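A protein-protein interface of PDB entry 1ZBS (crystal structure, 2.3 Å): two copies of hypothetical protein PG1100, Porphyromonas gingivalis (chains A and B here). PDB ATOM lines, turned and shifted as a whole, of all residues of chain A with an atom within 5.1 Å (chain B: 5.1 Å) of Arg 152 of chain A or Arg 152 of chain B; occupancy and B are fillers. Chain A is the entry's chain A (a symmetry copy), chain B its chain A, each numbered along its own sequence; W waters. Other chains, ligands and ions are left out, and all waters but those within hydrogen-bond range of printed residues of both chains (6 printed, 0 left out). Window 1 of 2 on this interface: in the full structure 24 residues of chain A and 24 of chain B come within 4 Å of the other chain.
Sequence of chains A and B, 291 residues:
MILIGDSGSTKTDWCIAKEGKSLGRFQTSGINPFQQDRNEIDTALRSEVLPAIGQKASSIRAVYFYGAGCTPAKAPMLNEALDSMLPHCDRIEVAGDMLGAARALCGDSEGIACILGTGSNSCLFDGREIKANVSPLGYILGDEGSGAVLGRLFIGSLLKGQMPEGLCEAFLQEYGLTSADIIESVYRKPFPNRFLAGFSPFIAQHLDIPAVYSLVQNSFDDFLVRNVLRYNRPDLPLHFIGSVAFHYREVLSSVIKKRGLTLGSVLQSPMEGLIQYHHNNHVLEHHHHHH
Printed residues of chain A that touch a printed residue of chain B: Tyr 139, Ile 140, Leu 141, Arg 152, Ile 155 and Gly 156.
Hydrophobic or aromatic side chains of chain B that line the printed part of chain A: Tyr 139, Ile 140, Leu 141 and Ile 155.
Among the printed residues, 12 pairs touch across the chains.
Among the printed residues, no Asp or Glu carboxylate lies within 4 Å of a Lys or Arg side-chain nitrogen of the other chain.
Water W1 lies within hydrogen-bond range of O of Arg 152 of chain A (2.8 Å) and O of Leu 141 of chain B (2.8 Å).
Water W4 lies within hydrogen-bond range of the backbone carbonyl oxygen (O) of Arg 152 of chain B and the backbone carbonyl oxygen (O) of Leu 141 of chain A.
Water W5 bridges NH1 of Arg 152 of chain A and NH1 of Arg 152 of chain B.
Water W6 lies within hydrogen-bond range of the guanidinium group (NH1) of Arg 152 of chain B and the guanidinium group (NH1) of Arg 152 of chain A.
Water W3 lies within hydrogen-bond range of O of Leu 141 of chain B and O of Gly 156 of chain A.
Water W2 bridges O of Leu 141 of chain A and O of Gly 156 of chain B.
Tyr 139 of chain A touches Ile 140 of chain B, and with the chains exchanged Ile 140 of chain A touches Tyr 139 of chain B.
Leu 141 of chain A touches Ile 155 of chain B, and with the chains exchanged Ile 155 of chain A touches Leu 141 of chain B.
Leu 141 of chain A touches Gly 156 of chain B, and with the chains exchanged Gly 156 of chain A touches Leu 141 of chain B.
Arg 152 of chain A touches its own counterpart, Arg 152 of chain B.
15 positions are printed for both chains.
Of the 12 pairs that touch across the chains among the printed residues, 12 have their exchanged pair printed and touching as well.
Phe 154 of chain A touches none of the printed residues of chain B.
Of the printed residues of chain B, Gly 156 of chain A touches Leu 141 (3.6 Å).
Arg 152 of chain B touches just these residues of chain A: Ile 140, Leu 141 and Arg 152.
Of the printed residues of chain A, Gly 156 of chain B touches Leu 141.
The backbone carbonyl oxygen (O) of Tyr 139 of chain B is in hydrogen-bond range of the guanidinium group (NE) of Arg 152 of chain B, 2.9 Å away.
NE of Arg 152 of chain A is in hydrogen-bond range of O of Tyr 139 of chain A, at 2.9 Å.
Ile 140 of chain B touches Tyr 139 of chain A.
Ile 140 of chain A touches Tyr 139 of chain B.
Ile 140 of chain A touches Arg 152 of chain B.
Leu 141 of chain A touches Arg 152 of chain B.
Ile 155 of chain B touches Leu 141 of chain A.
Arg 152 of chain A touches Ile 140 of chain B.
CB of Arg 152 of chain A touches CD2 of Leu 141 of chain B, 3.7 Å away.
NH1 of Arg 152 of chain A touches NH1 of Arg 152 of chain B (3.9 Å).
CD1 of Leu 141 of chain B touches CD1 of Ile 155 of chain A, 3.3 Å away.
O of Leu 141 of chain B touches CA of Gly 156 of chain A (3.6 Å).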
ATOM      1  N   TYR A 139      19.702 -17.249   5.999  1.00  0.00           N
ATOM      2  CA  TYR A 139      20.465 -17.748   7.139  1.00  0.00           C
ATOM      3  C   TYR A 139      19.812 -17.504   8.492  1.00  0.00           C
ATOM      4  O   TYR A 139      20.240 -18.063   9.507  1.00  0.00           O
ATOM      5  CB  TYR A 139      21.878 -17.159   7.150  1.00  0.00           C
ATOM      6  CG  TYR A 139      21.968 -15.769   7.732  1.00  0.00           C
ATOM      7  CD1 TYR A 139      21.471 -14.667   7.047  1.00  0.00           C
ATOM      8  CD2 TYR A 139      22.517 -15.564   8.988  1.00  0.00           C
ATOM      9  CE1 TYR A 139      21.518 -13.385   7.606  1.00  0.00           C
ATOM     10  CE2 TYR A 139      22.570 -14.295   9.559  1.00  0.00           C
ATOM     11  CZ  TYR A 139      22.068 -13.212   8.865  1.00  0.00           C
ATOM     12  OH  TYR A 139      22.099 -11.960   9.452  1.00  0.00           O
ATOM     13  N   ILE A 140      18.780 -16.672   8.529  1.00  0.00           N
ATOM     14  CA  ILE A 140      18.110 -16.436   9.797  1.00  0.00           C
ATOM     15  C   ILE A 140      16.859 -17.306   9.933  1.00  0.00           C
ATOM     16  O   ILE A 140      16.665 -17.965  10.960  1.00  0.00           O
ATOM     17  CB  ILE A 140      17.741 -14.935   9.991  1.00  0.00           C
ATOM     18  CG1 ILE A 140      19.027 -14.093  10.096  1.00  0.00           C
ATOM     19  CG2 ILE A 140      16.907 -14.753  11.264  1.00  0.00           C
ATOM     20  CD1 ILE A 140      18.779 -12.593  10.253  1.00  0.00           C
ATOM     21  N   LEU A 141      16.027 -17.348   8.901  1.00  0.00           N
ATOM     22  CA  LEU A 141      14.794 -18.155   8.968  1.00  0.00           C
ATOM     23  C   LEU A 141      14.904 -19.582   8.430  1.00  0.00           C
ATOM     24  O   LEU A 141      14.067 -20.429   8.744  1.00  0.00           O
ATOM     25  CB  LEU A 141      13.667 -17.450   8.217  1.00  0.00           C
ATOM     26  CG  LEU A 141      13.278 -16.083   8.762  1.00  0.00           C
ATOM     27  CD1 LEU A 141      12.275 -15.417   7.827  1.00  0.00           C
ATOM     28  CD2 LEU A 141      12.702 -16.249  10.161  1.00  0.00           C
ATOM     29  N   GLY A 142      15.923 -19.835   7.609  1.00  0.00           N
ATOM     30  CA  GLY A 142      16.088 -21.155   7.029  1.00  0.00           C
ATOM     31  C   GLY A 142      17.507 -21.544   6.656  1.00  0.00           C
ATOM     32  O   GLY A 142      18.378 -21.658   7.520  1.00  0.00           O
ATOM     33  N   ALA A 148      26.368 -20.730   6.510  1.00  0.00           N
ATOM     34  CA  ALA A 148      26.055 -19.611   7.387  1.00  0.00           C
ATOM     35  C   ALA A 148      25.328 -20.158   8.606  1.00  0.00           C
ATOM     36  O   ALA A 148      25.576 -19.727   9.729  1.00  0.00           O
ATOM     37  CB  ALA A 148      25.188 -18.583   6.671  1.00  0.00           C
ATOM     38  N   VAL A 149      24.439 -21.121   8.395  1.00  0.00           N
ATOM     39  CA  VAL A 149      23.715 -21.667   9.522  1.00  0.00           C
ATOM     40  C   VAL A 149      24.609 -22.524  10.402  1.00  0.00           C
ATOM     41  O   VAL A 149      24.544 -22.426  11.625  1.00  0.00           O
ATOM     42  CB  VAL A 149      22.485 -22.444   9.065  1.00  0.00           C
ATOM     43  CG1 VAL A 149      21.830 -23.139  10.256  1.00  0.00           C
ATOM     44  CG2 VAL A 149      21.498 -21.477   8.431  1.00  0.00           C
ATOM     45  N   LEU A 150      25.451 -23.354   9.794  1.00  0.00           N
ATOM     46  CA  LEU A 150      26.378 -24.177  10.571  1.00  0.00           C
ATOM     47  C   LEU A 150      27.191 -23.228  11.438  1.00  0.00           C
ATOM     48  O   LEU A 150      27.412 -23.474  12.620  1.00  0.00           O
ATOM     49  CB  LEU A 150      27.325 -24.940   9.647  1.00  0.00           C
ATOM     50  CG  LEU A 150      26.705 -26.023   8.757  1.00  0.00           C
ATOM     51  CD1 LEU A 150      27.813 -26.679   7.912  1.00  0.00           C
ATOM     52  CD2 LEU A 150      26.000 -27.055   9.623  1.00  0.00           C
ATOM     53  N   GLY A 151      27.623 -22.128  10.832  1.00  0.00           N
ATOM     54  CA  GLY A 151      28.401 -21.139  11.554  1.00  0.00           C
ATOM     55  C   GLY A 151      27.697 -20.512  12.752  1.00  0.00           C
ATOM     56  O   GLY A 151      28.275 -20.454  13.837  1.00  0.00           O
ATOM     57  N   ARG A 152      26.465 -20.036  12.591  1.00  0.00           N
ATOM     58  CA  ARG A 152      25.813 -19.426  13.745  1.00  0.00           C
ATOM     59  C   ARG A 152      25.480 -20.462  14.816  1.00  0.00           C
ATOM     60  O   ARG A 152      25.575 -20.174  16.014  1.00  0.00           O
ATOM     61  CB  ARG A 152      24.554 -18.645  13.358  1.00  0.00           C
ATOM     62  CG  ARG A 152      23.371 -19.471  12.921  1.00  0.00           C
ATOM     63  CD  ARG A 152      22.093 -18.647  13.059  1.00  0.00           C
ATOM     64  NE  ARG A 152      21.092 -19.061  12.089  1.00  0.00           N
ATOM     65  CZ  ARG A 152      20.180 -19.999  12.297  1.00  0.00           C
ATOM     66  NH1 ARG A 152      20.124 -20.630  13.459  1.00  0.00           N
ATOM     67  NH2 ARG A 152      19.328 -20.309  11.330  1.00  0.00           N
ATOM     68  N   LEU A 153      25.099 -21.664  14.396  1.00  0.00           N
ATOM     69  CA  LEU A 153      24.799 -22.713  15.361  1.00  0.00           C
ATOM     70  C   LEU A 153      26.082 -22.996  16.142  1.00  0.00           C
ATOM     71  O   LEU A 153      26.102 -22.985  17.376  1.00  0.00           O
ATOM     72  CB  LEU A 153      24.315 -23.994  14.653  1.00  0.00           C
ATOM     73  CG  LEU A 153      22.940 -23.948  13.976  1.00  0.00           C
ATOM     74  CD1 LEU A 153      22.663 -25.279  13.277  1.00  0.00           C
ATOM     75  CD2 LEU A 153      21.841 -23.668  15.015  1.00  0.00           C
ATOM     76  N   PHE A 154      27.165 -23.223  15.410  1.00  0.00           N
ATOM     77  CA  PHE A 154      28.447 -23.520  16.030  1.00  0.00           C
ATOM     78  C   PHE A 154      28.959 -22.461  17.019  1.00  0.00           C
ATOM     79  O   PHE A 154      29.219 -22.783  18.179  1.00  0.00           O
ATOM     80  CB  PHE A 154      29.493 -23.763  14.949  1.00  0.00           C
ATOM     81  CG  PHE A 154      30.846 -24.089  15.493  1.00  0.00           C
ATOM     82  CD1 PHE A 154      31.084 -25.303  16.120  1.00  0.00           C
ATOM     83  CD2 PHE A 154      31.880 -23.173  15.392  1.00  0.00           C
ATOM     84  CE1 PHE A 154      32.340 -25.595  16.634  1.00  0.00           C
ATOM     85  CE2 PHE A 154      33.136 -23.456  15.903  1.00  0.00           C
ATOM     86  CZ  PHE A 154      33.366 -24.668  16.524  1.00  0.00           C
ATOM     87  N   ILE A 155      29.107 -21.210  16.587  1.00  0.00           N
ATOM     88  CA  ILE A 155      29.620 -20.204  17.505  1.00  0.00           C
ATOM     89  C   ILE A 155      28.658 -19.973  18.680  1.00  0.00           C
ATOM     90  O   ILE A 155      29.084 -19.656  19.795  1.00  0.00           O
ATOM     91  CB  ILE A 155      29.979 -18.860  16.771  1.00  0.00           C
ATOM     92  CG1 ILE A 155      28.745 -18.026  16.517  1.00  0.00           C
ATOM     93  CG2 ILE A 155      30.681 -19.146  15.449  1.00  0.00           C
ATOM     94  CD1 ILE A 155      28.537 -16.999  17.604  1.00  0.00           C
ATOM     95  N   GLY A 156      27.364 -20.169  18.447  1.00  0.00           N
ATOM     96  CA  GLY A 156      26.394 -19.989  19.516  1.00  0.00           C
ATOM     97  C   GLY A 156      26.678 -20.963  20.650  1.00  0.00           C
ATOM     98  O   GLY A 156      26.907 -20.560  21.793  1.00  0.00           O
ATOM     99  N   SER A 157      26.676 -22.252  20.333  1.00  0.00           N
ATOM    100  CA  SER A 157      26.936 -23.267  21.343  1.00  0.00           C
ATOM    101  C   SER A 157      28.351 -23.140  21.898  1.00  0.00           C
ATOM    102  O   SER A 157      28.595 -23.368  23.082  1.00  0.00           O
ATOM    103  CB  SER A 157      26.749 -24.654  20.743  1.00  0.00           C
ATOM    104  OG  SER A 157      27.615 -24.802  19.640  1.00  0.00           O
ATOM    105  N   LEU A 196      29.582 -15.400   9.022  1.00  0.00           N
ATOM    106  CA  LEU A 196      29.253 -16.654   9.681  1.00  0.00           C
ATOM    107  C   LEU A 196      29.695 -17.908   8.912  1.00  0.00           C
ATOM    108  O   LEU A 196      30.183 -18.865   9.515  1.00  0.00           O
ATOM    109  CB  LEU A 196      27.744 -16.718   9.947  1.00  0.00           C
ATOM    110  CG  LEU A 196      27.232 -15.825  11.083  1.00  0.00           C
ATOM    111  CD1 LEU A 196      25.716 -15.895  11.138  1.00  0.00           C
ATOM    112  CD2 LEU A 196      27.841 -16.281  12.414  1.00  0.00           C
ATOM    113  N   TYR B 139      19.188 -12.345  19.089  1.00  0.00           N
ATOM    114  CA  TYR B 139      18.199 -13.207  18.449  1.00  0.00           C
ATOM    115  C   TYR B 139      18.747 -14.075  17.326  1.00  0.00           C
ATOM    116  O   TYR B 139      18.072 -14.996  16.856  1.00  0.00           O
ATOM    117  CB  TYR B 139      17.021 -12.383  17.919  1.00  0.00           C
ATOM    118  CG  TYR B 139      17.273 -11.726  16.584  1.00  0.00           C
ATOM    119  CD1 TYR B 139      18.135 -10.643  16.464  1.00  0.00           C
ATOM    120  CD2 TYR B 139      16.677 -12.215  15.432  1.00  0.00           C
ATOM    121  CE1 TYR B 139      18.400 -10.061  15.219  1.00  0.00           C
ATOM    122  CE2 TYR B 139      16.930 -11.649  14.186  1.00  0.00           C
ATOM    123  CZ  TYR B 139      17.793 -10.576  14.086  1.00  0.00           C
ATOM    124  OH  TYR B 139      18.061 -10.037  12.841  1.00  0.00           O
ATOM    125  N   ILE B 140      19.965 -13.796  16.881  1.00  0.00           N
ATOM    126  CA  ILE B 140      20.536 -14.622  15.829  1.00  0.00           C
ATOM    127  C   ILE B 140      21.462 -15.692  16.407  1.00  0.00           C
ATOM    128  O   ILE B 140      21.349 -16.872  16.057  1.00  0.00           O
ATOM    129  CB  ILE B 140      21.298 -13.770  14.770  1.00  0.00           C
ATOM    130  CG1 ILE B 140      20.305 -12.863  14.021  1.00  0.00           C
ATOM    131  CG2 ILE B 140      22.010 -14.685  13.766  1.00  0.00           C
ATOM    132  CD1 ILE B 140      20.955 -11.954  12.978  1.00  0.00           C
ATOM    133  N   LEU B 141      22.352 -15.309  17.315  1.00  0.00           N
ATOM    134  CA  LEU B 141      23.286 -16.286  17.903  1.00  0.00           C
ATOM    135  C   LEU B 141      22.828 -16.940  19.208  1.00  0.00           C
ATOM    136  O   LEU B 141      23.349 -17.989  19.591  1.00  0.00           O
ATOM    137  CB  LEU B 141      24.641 -15.628  18.153  1.00  0.00           C
ATOM    138  CG  LEU B 141      25.347 -15.101  16.911  1.00  0.00           C
ATOM    139  CD1 LEU B 141      26.592 -14.319  17.313  1.00  0.00           C
ATOM    140  CD2 LEU B 141      25.699 -16.272  16.004  1.00  0.00           C
ATOM    141  N   GLY B 142      21.873 -16.310  19.890  1.00  0.00           N
ATOM    142  CA  GLY B 142      21.397 -16.844  21.153  1.00  0.00           C
ATOM    143  C   GLY B 142      19.974 -16.480  21.535  1.00  0.00           C
ATOM    144  O   GLY B 142      19.021 -16.859  20.852  1.00  0.00           O
ATOM    145  N   ALA B 148      11.789 -13.256  20.194  1.00  0.00           N
ATOM    146  CA  ALA B 148      12.314 -13.096  18.847  1.00  0.00           C
ATOM    147  C   ALA B 148      12.721 -14.470  18.335  1.00  0.00           C
ATOM    148  O   ALA B 148      12.490 -14.799  17.173  1.00  0.00           O
ATOM    149  CB  ALA B 148      13.512 -12.154  18.838  1.00  0.00           C
ATOM    150  N   VAL B 149      13.313 -15.284  19.200  1.00  0.00           N
ATOM    151  CA  VAL B 149      13.726 -16.598  18.757  1.00  0.00           C
ATOM    152  C   VAL B 149      12.536 -17.514  18.530  1.00  0.00           C
ATOM    153  O   VAL B 149      12.495 -18.236  17.536  1.00  0.00           O
ATOM    154  CB  VAL B 149      14.722 -17.221  19.730  1.00  0.00           C
ATOM    155  CG1 VAL B 149      15.020 -18.662  19.324  1.00  0.00           C
ATOM    156  CG2 VAL B 149      16.006 -16.408  19.708  1.00  0.00           C
ATOM    157  N   LEU B 150      11.559 -17.485  19.432  1.00  0.00           N
ATOM    158  CA  LEU B 150      10.359 -18.301  19.259  1.00  0.00           C
ATOM    159  C   LEU B 150       9.765 -17.933  17.907  1.00  0.00           C
ATOM    160  O   LEU B 150       9.359 -18.795  17.133  1.00  0.00           O
ATOM    161  CB  LEU B 150       9.335 -17.993  20.351  1.00  0.00           C
ATOM    162  CG  LEU B 150       9.709 -18.387  21.783  1.00  0.00           C
ATOM    163  CD1 LEU B 150       8.555 -18.006  22.730  1.00  0.00           C
ATOM    164  CD2 LEU B 150       9.992 -19.879  21.847  1.00  0.00           C
ATOM    165  N   GLY B 151       9.734 -16.635  17.631  1.00  0.00           N
ATOM    166  CA  GLY B 151       9.202 -16.157  16.368  1.00  0.00           C
ATOM    167  C   GLY B 151       9.925 -16.667  15.128  1.00  0.00           C
ATOM    168  O   GLY B 151       9.277 -17.145  14.197  1.00  0.00           O
ATOM    169  N   ARG B 152      11.252 -16.576  15.080  1.00  0.00           N
ATOM    170  CA  ARG B 152      11.925 -17.055  13.878  1.00  0.00           C
ATOM    171  C   ARG B 152      11.832 -18.573  13.747  1.00  0.00           C
ATOM    172  O   ARG B 152      11.697 -19.097  12.636  1.00  0.00           O
ATOM    173  CB  ARG B 152      13.390 -16.611  13.813  1.00  0.00           C
ATOM    174  CG  ARG B 152      14.325 -17.268  14.796  1.00  0.00           C
ATOM    175  CD  ARG B 152      15.764 -17.131  14.305  1.00  0.00           C
ATOM    176  NE  ARG B 152      16.700 -17.102  15.417  1.00  0.00           N
ATOM    177  CZ  ARG B 152      17.277 -18.170  15.946  1.00  0.00           C
ATOM    178  NH1 ARG B 152      17.026 -19.375  15.461  1.00  0.00           N
ATOM    179  NH2 ARG B 152      18.101 -18.026  16.975  1.00  0.00           N
ATOM    180  N   LEU B 153      11.894 -19.282  14.870  1.00  0.00           N
ATOM    181  CA  LEU B 153      11.776 -20.733  14.825  1.00  0.00           C
ATOM    182  C   LEU B 153      10.390 -21.063  14.270  1.00  0.00           C
ATOM    183  O   LEU B 153      10.243 -21.829  13.314  1.00  0.00           O
ATOM    184  CB  LEU B 153      11.943 -21.345  16.230  1.00  0.00           C
ATOM    185  CG  LEU B 153      13.336 -21.279  16.865  1.00  0.00           C
ATOM    186  CD1 LEU B 153      13.292 -21.873  18.273  1.00  0.00           C
ATOM    187  CD2 LEU B 153      14.354 -22.051  16.007  1.00  0.00           C
ATOM    188  N   PHE B 154       9.371 -20.451  14.860  1.00  0.00           N
ATOM    189  CA  PHE B 154       8.001 -20.688  14.437  1.00  0.00           C
ATOM    190  C   PHE B 154       7.712 -20.406  12.954  1.00  0.00           C
ATOM    191  O   PHE B 154       7.250 -21.296  12.239  1.00  0.00           O
ATOM    192  CB  PHE B 154       7.049 -19.878  15.309  1.00  0.00           C
ATOM    193  CG  PHE B 154       5.610 -20.068  14.955  1.00  0.00           C
ATOM    194  CD1 PHE B 154       4.967 -21.269  15.217  1.00  0.00           C
ATOM    195  CD2 PHE B 154       4.899 -19.048  14.344  1.00  0.00           C
ATOM    196  CE1 PHE B 154       3.634 -21.443  14.874  1.00  0.00           C
ATOM    197  CE2 PHE B 154       3.569 -19.214  13.997  1.00  0.00           C
ATOM    198  CZ  PHE B 154       2.936 -20.412  14.263  1.00  0.00           C
ATOM    199  N   ILE B 155       7.976 -19.190  12.478  1.00  0.00           N
ATOM    200  CA  ILE B 155       7.680 -18.900  11.083  1.00  0.00           C
ATOM    201  C   ILE B 155       8.539 -19.753  10.136  1.00  0.00           C
ATOM    202  O   ILE B 155       8.106 -20.108   9.036  1.00  0.00           O
ATOM    203  CB  ILE B 155       7.802 -17.366  10.758  1.00  0.00           C
ATOM    204  CG1 ILE B 155       9.244 -16.961  10.555  1.00  0.00           C
ATOM    205  CG2 ILE B 155       7.192 -16.533  11.878  1.00  0.00           C
ATOM    206  CD1 ILE B 155       9.623 -16.968   9.094  1.00  0.00           C
ATOM    207  N   GLY B 156       9.738 -20.119  10.577  1.00  0.00           N
ATOM    208  CA  GLY B 156      10.600 -20.945   9.745  1.00  0.00           C
ATOM    209  C   GLY B 156       9.931 -22.281   9.461  1.00  0.00           C
ATOM    210  O   GLY B 156       9.707 -22.648   8.306  1.00  0.00           O
ATOM    211  N   SER B 157       9.596 -23.007  10.520  1.00  0.00           N
ATOM    212  CA  SER B 157       8.950 -24.302  10.360  1.00  0.00           C
ATOM    213  C   SER B 157       7.580 -24.155   9.705  1.00  0.00           C
ATOM    214  O   SER B 157       7.157 -24.998   8.915  1.00  0.00           O
ATOM    215  CB  SER B 157       8.792 -24.973  11.718  1.00  0.00           C
ATOM    216  OG  SER B 157       8.042 -24.134  12.566  1.00  0.00           O
ATOM    217  N   LEU B 196       9.995 -10.089  14.556  1.00  0.00           N
ATOM    218  CA  LEU B 196       9.878 -11.501  14.878  1.00  0.00           C
ATOM    219  C   LEU B 196       9.179 -11.790  16.214  1.00  0.00           C
ATOM    220  O   LEU B 196       8.374 -12.720  16.306  1.00  0.00           O
ATOM    221  CB  LEU B 196      11.268 -12.150  14.874  1.00  0.00           C
ATOM    222  CG  LEU B 196      11.891 -12.373  13.491  1.00  0.00           C
ATOM    223  CD1 LEU B 196      13.309 -12.894  13.654  1.00  0.00           C
ATOM    224  CD2 LEU B 196      11.040 -13.369  12.695  1.00  0.00           C
HETATM  225  O   HOH W   1      23.702 -20.390  18.129  1.00  0.00           O
HETATM  226  O   HOH W   2      12.968 -23.236   7.891  1.00  0.00           O
HETATM  227  O   HOH W   3      23.678 -19.783  22.137  1.00  0.00           O
HETATM  228  O   HOH W   4      13.194 -21.129  11.348  1.00  0.00           O
HETATM  229  O   HOH W   5      17.428 -22.069  13.687  1.00  0.00           O
HETATM  230  O   HOH W   6      19.155 -21.330  16.482  1.00  0.00           O
